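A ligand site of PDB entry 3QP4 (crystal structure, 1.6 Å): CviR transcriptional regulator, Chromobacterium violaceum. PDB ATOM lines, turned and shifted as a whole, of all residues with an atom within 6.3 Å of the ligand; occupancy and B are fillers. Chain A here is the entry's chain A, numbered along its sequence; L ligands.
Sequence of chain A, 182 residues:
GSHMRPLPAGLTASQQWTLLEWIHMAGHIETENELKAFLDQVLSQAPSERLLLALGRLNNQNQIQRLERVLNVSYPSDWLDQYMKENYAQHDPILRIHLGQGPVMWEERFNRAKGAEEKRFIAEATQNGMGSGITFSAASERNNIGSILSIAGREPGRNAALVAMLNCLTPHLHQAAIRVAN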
ATOM      1  N   LEU A  52      15.101 -24.098   1.646  1.00  0.00           N
ATOM      2  CA  LEU A  52      13.690 -24.377   1.847  1.00  0.00           C
ATOM      3  C   LEU A  52      12.838 -23.471   0.957  1.00  0.00           C
ATOM      4  O   LEU A  52      13.166 -22.299   0.779  1.00  0.00           O
ATOM      5  CB  LEU A  52      13.320 -24.189   3.331  1.00  0.00           C
ATOM      6  CG  LEU A  52      11.875 -24.459   3.775  1.00  0.00           C
ATOM      7  CD1 LEU A  52      11.833 -25.130   5.146  1.00  0.00           C
ATOM      8  CD2 LEU A  52      11.013 -23.183   3.777  1.00  0.00           C
ATOM      9  N   ALA A  54       8.745 -22.237   0.443  1.00  0.00           N
ATOM     10  CA  ALA A  54       7.385 -22.278   1.012  1.00  0.00           C
ATOM     11  C   ALA A  54       6.428 -21.450   0.201  1.00  0.00           C
ATOM     12  O   ALA A  54       6.788 -20.400  -0.337  1.00  0.00           O
ATOM     13  CB  ALA A  54       7.385 -21.852   2.479  1.00  0.00           C
ATOM     14  N   LEU A  67       0.704 -20.546   5.867  1.00  0.00           N
ATOM     15  CA  LEU A  67       1.556 -21.420   5.052  1.00  0.00           C
ATOM     16  C   LEU A  67       0.721 -22.521   4.413  1.00  0.00           C
ATOM     17  O   LEU A  67      -0.012 -23.227   5.108  1.00  0.00           O
ATOM     18  CB  LEU A  67       2.687 -22.005   5.886  1.00  0.00           C
ATOM     19  CG  LEU A  67       3.765 -21.025   6.325  1.00  0.00           C
ATOM     20  CD1 LEU A  67       4.569 -21.583   7.512  1.00  0.00           C
ATOM     21  CD2 LEU A  67       4.691 -20.661   5.164  1.00  0.00           C
ATOM     22  N   VAL A  70       5.069 -26.391   2.456  1.00  0.00           N
ATOM     23  CA  VAL A  70       6.482 -26.232   2.739  1.00  0.00           C
ATOM     24  C   VAL A  70       7.211 -27.354   2.040  1.00  0.00           C
ATOM     25  O   VAL A  70       6.869 -28.527   2.208  1.00  0.00           O
ATOM     26  CB  VAL A  70       6.751 -26.258   4.255  1.00  0.00           C
ATOM     27  CG1 VAL A  70       8.238 -26.202   4.545  1.00  0.00           C
ATOM     28  CG2 VAL A  70       6.005 -25.123   4.947  1.00  0.00           C
ATOM     29  N   TYR A  75      16.899 -28.029   4.997  1.00  0.00           N
ATOM     30  CA  TYR A  75      16.940 -27.568   6.390  1.00  0.00           C
ATOM     31  C   TYR A  75      17.037 -28.795   7.296  1.00  0.00           C
ATOM     32  O   TYR A  75      16.419 -29.812   7.008  1.00  0.00           O
ATOM     33  CB  TYR A  75      15.691 -26.769   6.760  1.00  0.00           C
ATOM     34  CG  TYR A  75      15.728 -25.297   6.451  1.00  0.00           C
ATOM     35  CD1 TYR A  75      14.939 -24.416   7.173  1.00  0.00           C
ATOM     36  CD2 TYR A  75      16.525 -24.792   5.429  1.00  0.00           C
ATOM     37  CE1 TYR A  75      14.928 -23.054   6.895  1.00  0.00           C
ATOM     38  CE2 TYR A  75      16.533 -23.419   5.152  1.00  0.00           C
ATOM     39  CZ  TYR A  75      15.728 -22.563   5.871  1.00  0.00           C
ATOM     40  OH  TYR A  75      15.715 -21.214   5.669  1.00  0.00           O
ATOM     41  N   TRP A  79      15.733 -28.916  13.321  1.00  0.00           N
ATOM     42  CA  TRP A  79      15.426 -27.478  13.365  1.00  0.00           C
ATOM     43  C   TRP A  79      13.949 -27.226  12.994  1.00  0.00           C
ATOM     44  O   TRP A  79      13.269 -26.412  13.637  1.00  0.00           O
ATOM     45  CB  TRP A  79      16.361 -26.673  12.456  1.00  0.00           C
ATOM     46  CG  TRP A  79      15.962 -25.229  12.315  1.00  0.00           C
ATOM     47  CD1 TRP A  79      15.562 -24.588  11.153  1.00  0.00           C
ATOM     48  CD2 TRP A  79      15.869 -24.245  13.361  1.00  0.00           C
ATOM     49  NE1 TRP A  79      15.243 -23.287  11.425  1.00  0.00           N
ATOM     50  CE2 TRP A  79      15.440 -23.041  12.760  1.00  0.00           C
ATOM     51  CE3 TRP A  79      16.140 -24.262  14.740  1.00  0.00           C
ATOM     52  CZ2 TRP A  79      15.246 -21.868  13.489  1.00  0.00           C
ATOM     53  CZ3 TRP A  79      15.932 -23.090  15.460  1.00  0.00           C
ATOM     54  CH2 TRP A  79      15.503 -21.912  14.841  1.00  0.00           C
ATOM     55  N   LEU A  80      13.466 -27.912  11.967  1.00  0.00           N
ATOM     56  CA  LEU A  80      12.074 -27.751  11.554  1.00  0.00           C
ATOM     57  C   LEU A  80      11.099 -28.289  12.604  1.00  0.00           C
ATOM     58  O   LEU A  80      10.076 -27.661  12.868  1.00  0.00           O
ATOM     59  CB  LEU A  80      11.815 -28.403  10.205  1.00  0.00           C
ATOM     60  CG  LEU A  80      12.415 -27.714   8.990  1.00  0.00           C
ATOM     61  CD1 LEU A  80      11.909 -28.404   7.750  1.00  0.00           C
ATOM     62  CD2 LEU A  80      12.045 -26.231   8.956  1.00  0.00           C
ATOM     63  N   TYR A  83      10.994 -25.685  15.220  1.00  0.00           N
ATOM     64  CA  TYR A  83      10.328 -24.506  14.701  1.00  0.00           C
ATOM     65  C   TYR A  83       8.809 -24.672  14.841  1.00  0.00           C
ATOM     66  O   TYR A  83       8.106 -23.751  15.259  1.00  0.00           O
ATOM     67  CB  TYR A  83      10.719 -24.335  13.236  1.00  0.00           C
ATOM     68  CG  TYR A  83      10.408 -22.999  12.601  1.00  0.00           C
ATOM     69  CD1 TYR A  83      11.417 -22.085  12.328  1.00  0.00           C
ATOM     70  CD2 TYR A  83       9.101 -22.657  12.247  1.00  0.00           C
ATOM     71  CE1 TYR A  83      11.131 -20.852  11.719  1.00  0.00           C
ATOM     72  CE2 TYR A  83       8.801 -21.436  11.650  1.00  0.00           C
ATOM     73  CZ  TYR A  83       9.812 -20.542  11.368  1.00  0.00           C
ATOM     74  OH  TYR A  83       9.500 -19.346  10.780  1.00  0.00           O
ATOM     75  N   MET A  84       8.338 -25.862  14.501  1.00  0.00           N
ATOM     76  CA  MET A  84       6.928 -26.220  14.648  1.00  0.00           C
ATOM     77  C   MET A  84       6.492 -26.306  16.116  1.00  0.00           C
ATOM     78  O   MET A  84       5.508 -25.685  16.509  1.00  0.00           O
ATOM     79  CB  MET A  84       6.646 -27.516  13.911  1.00  0.00           C
ATOM     80  CG  MET A  84       6.777 -27.398  12.414  1.00  0.00           C
ATOM     81  SD  MET A  84       6.218 -28.855  11.526  1.00  0.00           S
ATOM     82  CE  MET A  84       7.721 -29.830  11.452  1.00  0.00           C
ATOM     83  N   ALA A  89       6.957 -19.718  13.920  1.00  0.00           N
ATOM     84  CA  ALA A  89       6.325 -19.006  12.803  1.00  0.00           C
ATOM     85  C   ALA A  89       5.803 -17.645  13.252  1.00  0.00           C
ATOM     86  O   ALA A  89       5.784 -16.696  12.480  1.00  0.00           O
ATOM     87  CB  ALA A  89       5.184 -19.842  12.180  1.00  0.00           C
ATOM     88  N   ASP A  92       9.412 -15.430  13.903  1.00  0.00           N
ATOM     89  CA  ASP A  92      10.494 -15.397  12.931  1.00  0.00           C
ATOM     90  C   ASP A  92      10.322 -14.157  12.041  1.00  0.00           C
ATOM     91  O   ASP A  92       9.365 -14.078  11.288  1.00  0.00           O
ATOM     92  CB  ASP A  92      10.450 -16.687  12.101  1.00  0.00           C
ATOM     93  CG  ASP A  92      11.500 -16.748  11.003  1.00  0.00           C
ATOM     94  OD1 ASP A  92      12.271 -15.770  10.846  1.00  0.00           O
ATOM     95  OD2 ASP A  92      11.532 -17.786  10.319  1.00  0.00           O
ATOM     96  N   PRO A  93      11.259 -13.193  12.115  1.00  0.00           N
ATOM     97  CA  PRO A  93      11.171 -11.982  11.311  1.00  0.00           C
ATOM     98  C   PRO A  93      11.067 -12.275   9.806  1.00  0.00           C
ATOM     99  O   PRO A  93      10.494 -11.484   9.054  1.00  0.00           O
ATOM    100  CB  PRO A  93      12.480 -11.244  11.637  1.00  0.00           C
ATOM    101  CG  PRO A  93      12.917 -11.781  12.916  1.00  0.00           C
ATOM    102  CD  PRO A  93      12.474 -13.201  12.963  1.00  0.00           C
ATOM    103  N   ILE A  94      11.628 -13.390   9.372  1.00  0.00           N
ATOM    104  CA  ILE A  94      11.644 -13.702   7.940  1.00  0.00           C
ATOM    105  C   ILE A  94      10.229 -13.980   7.418  1.00  0.00           C
ATOM    106  O   ILE A  94       9.910 -13.682   6.260  1.00  0.00           O
ATOM    107  CB  ILE A  94      12.653 -14.863   7.616  1.00  0.00           C
ATOM    108  CG1 ILE A  94      14.074 -14.520   8.111  1.00  0.00           C
ATOM    109  CG2 ILE A  94      12.598 -15.244   6.121  1.00  0.00           C
ATOM    110  CD1 ILE A  94      14.539 -13.083   7.867  1.00  0.00           C
ATOM    111  N   LEU A  95       9.359 -14.522   8.274  1.00  0.00           N
ATOM    112  CA  LEU A  95       7.967 -14.752   7.877  1.00  0.00           C
ATOM    113  C   LEU A  95       7.114 -13.474   7.876  1.00  0.00           C
ATOM    114  O   LEU A  95       5.939 -13.516   7.488  1.00  0.00           O
ATOM    115  CB  LEU A  95       7.315 -15.867   8.706  1.00  0.00           C
ATOM    116  CG  LEU A  95       7.780 -17.312   8.462  1.00  0.00           C
ATOM    117  CD1 LEU A  95       6.833 -18.256   9.149  1.00  0.00           C
ATOM    118  CD2 LEU A  95       7.856 -17.663   6.987  1.00  0.00           C
ATOM    119  N   TRP A 106      19.265 -12.018   6.230  1.00  0.00           N
ATOM    120  CA  TRP A 106      18.743 -12.301   7.560  1.00  0.00           C
ATOM    121  C   TRP A 106      19.457 -11.481   8.623  1.00  0.00           C
ATOM    122  O   TRP A 106      18.805 -10.968   9.516  1.00  0.00           O
ATOM    123  CB  TRP A 106      18.872 -13.769   7.904  1.00  0.00           C
ATOM    124  CG  TRP A 106      18.107 -14.726   7.023  1.00  0.00           C
ATOM    125  CD1 TRP A 106      17.242 -14.421   5.996  1.00  0.00           C
ATOM    126  CD2 TRP A 106      18.140 -16.147   7.111  1.00  0.00           C
ATOM    127  NE1 TRP A 106      16.761 -15.589   5.434  1.00  0.00           N
ATOM    128  CE2 TRP A 106      17.290 -16.667   6.099  1.00  0.00           C
ATOM    129  CE3 TRP A 106      18.841 -17.052   7.947  1.00  0.00           C
ATOM    130  CZ2 TRP A 106      17.108 -18.044   5.903  1.00  0.00           C
ATOM    131  CZ3 TRP A 106      18.656 -18.415   7.753  1.00  0.00           C
ATOM    132  CH2 TRP A 106      17.796 -18.901   6.741  1.00  0.00           C
ATOM    133  N   PHE A 110      17.682  -9.360  11.309  1.00  0.00           N
ATOM    134  CA  PHE A 110      17.792  -9.785  12.705  1.00  0.00           C
ATOM    135  C   PHE A 110      18.346  -8.675  13.600  1.00  0.00           C
ATOM    136  O   PHE A 110      17.908  -8.499  14.742  1.00  0.00           O
ATOM    137  CB  PHE A 110      18.670 -11.029  12.829  1.00  0.00           C
ATOM    138  CG  PHE A 110      18.040 -12.280  12.279  1.00  0.00           C
ATOM    139  CD1 PHE A 110      16.704 -12.314  11.909  1.00  0.00           C
ATOM    140  CD2 PHE A 110      18.803 -13.444  12.150  1.00  0.00           C
ATOM    141  CE1 PHE A 110      16.138 -13.475  11.419  1.00  0.00           C
ATOM    142  CE2 PHE A 110      18.246 -14.603  11.656  1.00  0.00           C
ATOM    143  CZ  PHE A 110      16.913 -14.624  11.302  1.00  0.00           C
ATOM    144  N   PHE A 121      13.976 -16.061  19.492  1.00  0.00           N
ATOM    145  CA  PHE A 121      14.053 -16.826  18.260  1.00  0.00           C
ATOM    146  C   PHE A 121      15.416 -16.695  17.553  1.00  0.00           C
ATOM    147  O   PHE A 121      16.015 -17.676  17.109  1.00  0.00           O
ATOM    148  CB  PHE A 121      12.950 -16.397  17.301  1.00  0.00           C
ATOM    149  CG  PHE A 121      13.133 -16.947  15.918  1.00  0.00           C
ATOM    150  CD1 PHE A 121      12.826 -18.278  15.653  1.00  0.00           C
ATOM    151  CD2 PHE A 121      13.695 -16.155  14.910  1.00  0.00           C
ATOM    152  CE1 PHE A 121      13.051 -18.801  14.370  1.00  0.00           C
ATOM    153  CE2 PHE A 121      13.923 -16.691  13.625  1.00  0.00           C
ATOM    154  CZ  PHE A 121      13.605 -18.006  13.373  1.00  0.00           C
ATOM    155  N   ALA A 125      17.925 -19.581  16.581  1.00  0.00           N
ATOM    156  CA  ALA A 125      18.274 -19.805  15.194  1.00  0.00           C
ATOM    157  C   ALA A 125      19.792 -19.772  15.019  1.00  0.00           C
ATOM    158  O   ALA A 125      20.379 -20.637  14.355  1.00  0.00           O
ATOM    159  CB  ALA A 125      17.600 -18.770  14.314  1.00  0.00           C
ATOM    160  N   MET A 130      21.549 -20.995  11.823  1.00  0.00           N
ATOM    161  CA  MET A 130      20.564 -20.287  10.997  1.00  0.00           C
ATOM    162  C   MET A 130      20.569 -18.778  11.283  1.00  0.00           C
ATOM    163  O   MET A 130      19.568 -18.101  11.078  1.00  0.00           O
ATOM    164  CB  MET A 130      19.153 -20.888  11.236  1.00  0.00           C
ATOM    165  CG  MET A 130      19.073 -22.382  11.026  1.00  0.00           C
ATOM    166  SD  MET A 130      19.446 -22.797   9.298  1.00  0.00           S
ATOM    167  CE  MET A 130      17.856 -22.473   8.552  1.00  0.00           C
ATOM    168  N   GLY A 131      21.707 -18.251  11.740  1.00  0.00           N
ATOM    169  CA  GLY A 131      21.801 -16.849  12.073  1.00  0.00           C
ATOM    170  C   GLY A 131      22.031 -15.970  10.853  1.00  0.00           C
ATOM    171  O   GLY A 131      21.822 -14.743  10.922  1.00  0.00           O
ATOM    172  N   THR A 135      16.546 -14.652   1.976  1.00  0.00           N
ATOM    173  CA  THR A 135      15.225 -15.083   1.509  1.00  0.00           C
ATOM    174  C   THR A 135      14.762 -14.263   0.304  1.00  0.00           C
ATOM    175  O   THR A 135      14.707 -13.036   0.374  1.00  0.00           O
ATOM    176  CB  THR A 135      14.188 -15.049   2.653  1.00  0.00           C
ATOM    177  OG1 THR A 135      14.599 -15.977   3.669  1.00  0.00           O
ATOM    178  CG2 THR A 135      12.793 -15.446   2.157  1.00  0.00           C
ATOM    179  N   ILE A 148       8.317 -18.031  -0.812  1.00  0.00           N
ATOM    180  CA  ILE A 148       9.651 -17.680  -0.335  1.00  0.00           C
ATOM    181  C   ILE A 148      10.659 -18.784  -0.654  1.00  0.00           C
ATOM    182  O   ILE A 148      10.336 -19.975  -0.564  1.00  0.00           O
ATOM    183  CB  ILE A 148       9.688 -17.358   1.184  1.00  0.00           C
ATOM    184  CG1 ILE A 148       9.080 -18.490   2.033  1.00  0.00           C
ATOM    185  CG2 ILE A 148       9.014 -16.030   1.438  1.00  0.00           C
ATOM    186  CD1 ILE A 148       9.382 -18.329   3.562  1.00  0.00           C
ATOM    187  N   SER A 150      14.356 -19.712   0.762  1.00  0.00           N
ATOM    188  CA  SER A 150      15.313 -19.392   1.828  1.00  0.00           C
ATOM    189  C   SER A 150      16.541 -20.238   1.668  1.00  0.00           C
ATOM    190  O   SER A 150      16.461 -21.439   1.456  1.00  0.00           O
ATOM    191  CB  SER A 150      14.688 -19.651   3.193  1.00  0.00           C
ATOM    192  OG  SER A 150      13.796 -18.609   3.544  1.00  0.00           O
ATOM    193  N   ILE A 151      17.696 -19.588   1.779  1.00  0.00           N
ATOM    194  CA  ILE A 151      18.968 -20.300   1.775  1.00  0.00           C
ATOM    195  C   ILE A 151      19.792 -19.832   2.975  1.00  0.00           C
ATOM    196  O   ILE A 151      20.032 -18.635   3.139  1.00  0.00           O
ATOM    197  CB  ILE A 151      19.752 -20.089   0.449  1.00  0.00           C
ATOM    198  CG1 ILE A 151      18.903 -20.589  -0.722  1.00  0.00           C
ATOM    199  CG2 ILE A 151      21.082 -20.844   0.509  1.00  0.00           C
ATOM    200  CD1 ILE A 151      19.561 -20.398  -2.077  1.00  0.00           C
HETATM  201  N1  LIG L   1      13.368 -18.589   8.414  1.00  0.00           N
HETATM  202  C1  LIG L   1       5.501 -24.900   9.576  1.00  0.00           C
HETATM  203  O1  LIG L   1      13.750 -19.396   6.341  1.00  0.00           O
HETATM  204  C2  LIG L   1       6.902 -24.671  10.114  1.00  0.00           C
HETATM  205  O2  LIG L   1      15.792 -19.599  10.782  1.00  0.00           O
HETATM  206  C3  LIG L   1       7.973 -24.863   9.041  1.00  0.00           C
HETATM  207  O3  LIG L   1      14.384 -21.040   9.627  1.00  0.00           O
HETATM  208  C4  LIG L   1       8.123 -23.605   8.202  1.00  0.00           C
HETATM  209  C5  LIG L   1       9.475 -22.935   8.419  1.00  0.00           C
HETATM  210  C6  LIG L   1       9.629 -21.846   7.379  1.00  0.00           C
HETATM  211  C7  LIG L   1      10.784 -20.906   7.670  1.00  0.00           C
HETATM  212  C8  LIG L   1      10.816 -19.912   6.531  1.00  0.00           C
HETATM  213  C9  LIG L   1      11.550 -18.633   6.875  1.00  0.00           C
HETATM  214  C10 LIG L   1      12.994 -18.902   7.174  1.00  0.00           C
HETATM  215  C11 LIG L   1      14.730 -18.769   8.822  1.00  0.00           C
HETATM  216  C12 LIG L   1      15.245 -17.604   9.653  1.00  0.00           C
HETATM  217  C13 LIG L   1      16.211 -18.230  10.663  1.00  0.00           C
HETATM  218  C14 LIG L   1      14.902 -19.939   9.734  1.00  0.00           C
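The side-chain carboxylate (OD2) of Asp 92 lies within hydrogen-bond range of the side-chain hydroxyl (OH) of Tyr 83 (2.6 Å). N of Met 130 sits at hydrogen-bond distance from O of Ala 125. The side-chain hydroxyl (OG) of Ser 150 is in hydrogen-bond range of the side-chain hydroxyl (OG1) of Thr 135 (2.8 Å). The backbone NH (N) of Ile 148 sits at hydrogen-bond distance from the backbone carbonyl oxygen (O) of Ala 54, 2.9 Å away. The side-chain hydroxyl (OG1) of Thr 135 is in hydrogen-bond range of the indole nitrogen (NE1) of Trp 106 (2.8 Å). N of Ile 94 is in hydrogen-bond range of OD1 of Asp 92, at 2.9 Å. The backbone NH of Ser 150 sits at hydrogen-bond distance from the backbone carbonyl oxygen of Leu 52 (2.8 Å).
Merely in contact with the ligand: Tyr 83, Met 84, Ile 94, Leu 95, Trp 106, Phe 110, Phe 121, Ala 125, Met 130 and Ile 148. Hydrophobic or aromatic side chains that line the ligand: Tyr 75, Trp 79, Tyr 83, Met 84, Ile 94, Leu 95, Trp 106, Phe 110, Phe 121, Ala 125, Met 130 and Ile 148. The nearest printed residue that does not touch the ligand is Leu 67 (4.02 Å).
NE1 of Trp 79 lies within hydrogen-bond range of O3 of the ligand (3.0 Å). The side-chain hydroxyl (OG) of Ser 150 sits at hydrogen-bond distance from an oxygen (O1) of the ligand (2.9 Å). A nitrogen (N1) of the ligand sits at hydrogen-bond distance from the side-chain carboxylate (OD2) of Asp 92, 2.8 Å away. The side-chain hydroxyl (OH) of Tyr 75 sits at hydrogen-bond distance from an oxygen (O1) of the ligand.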
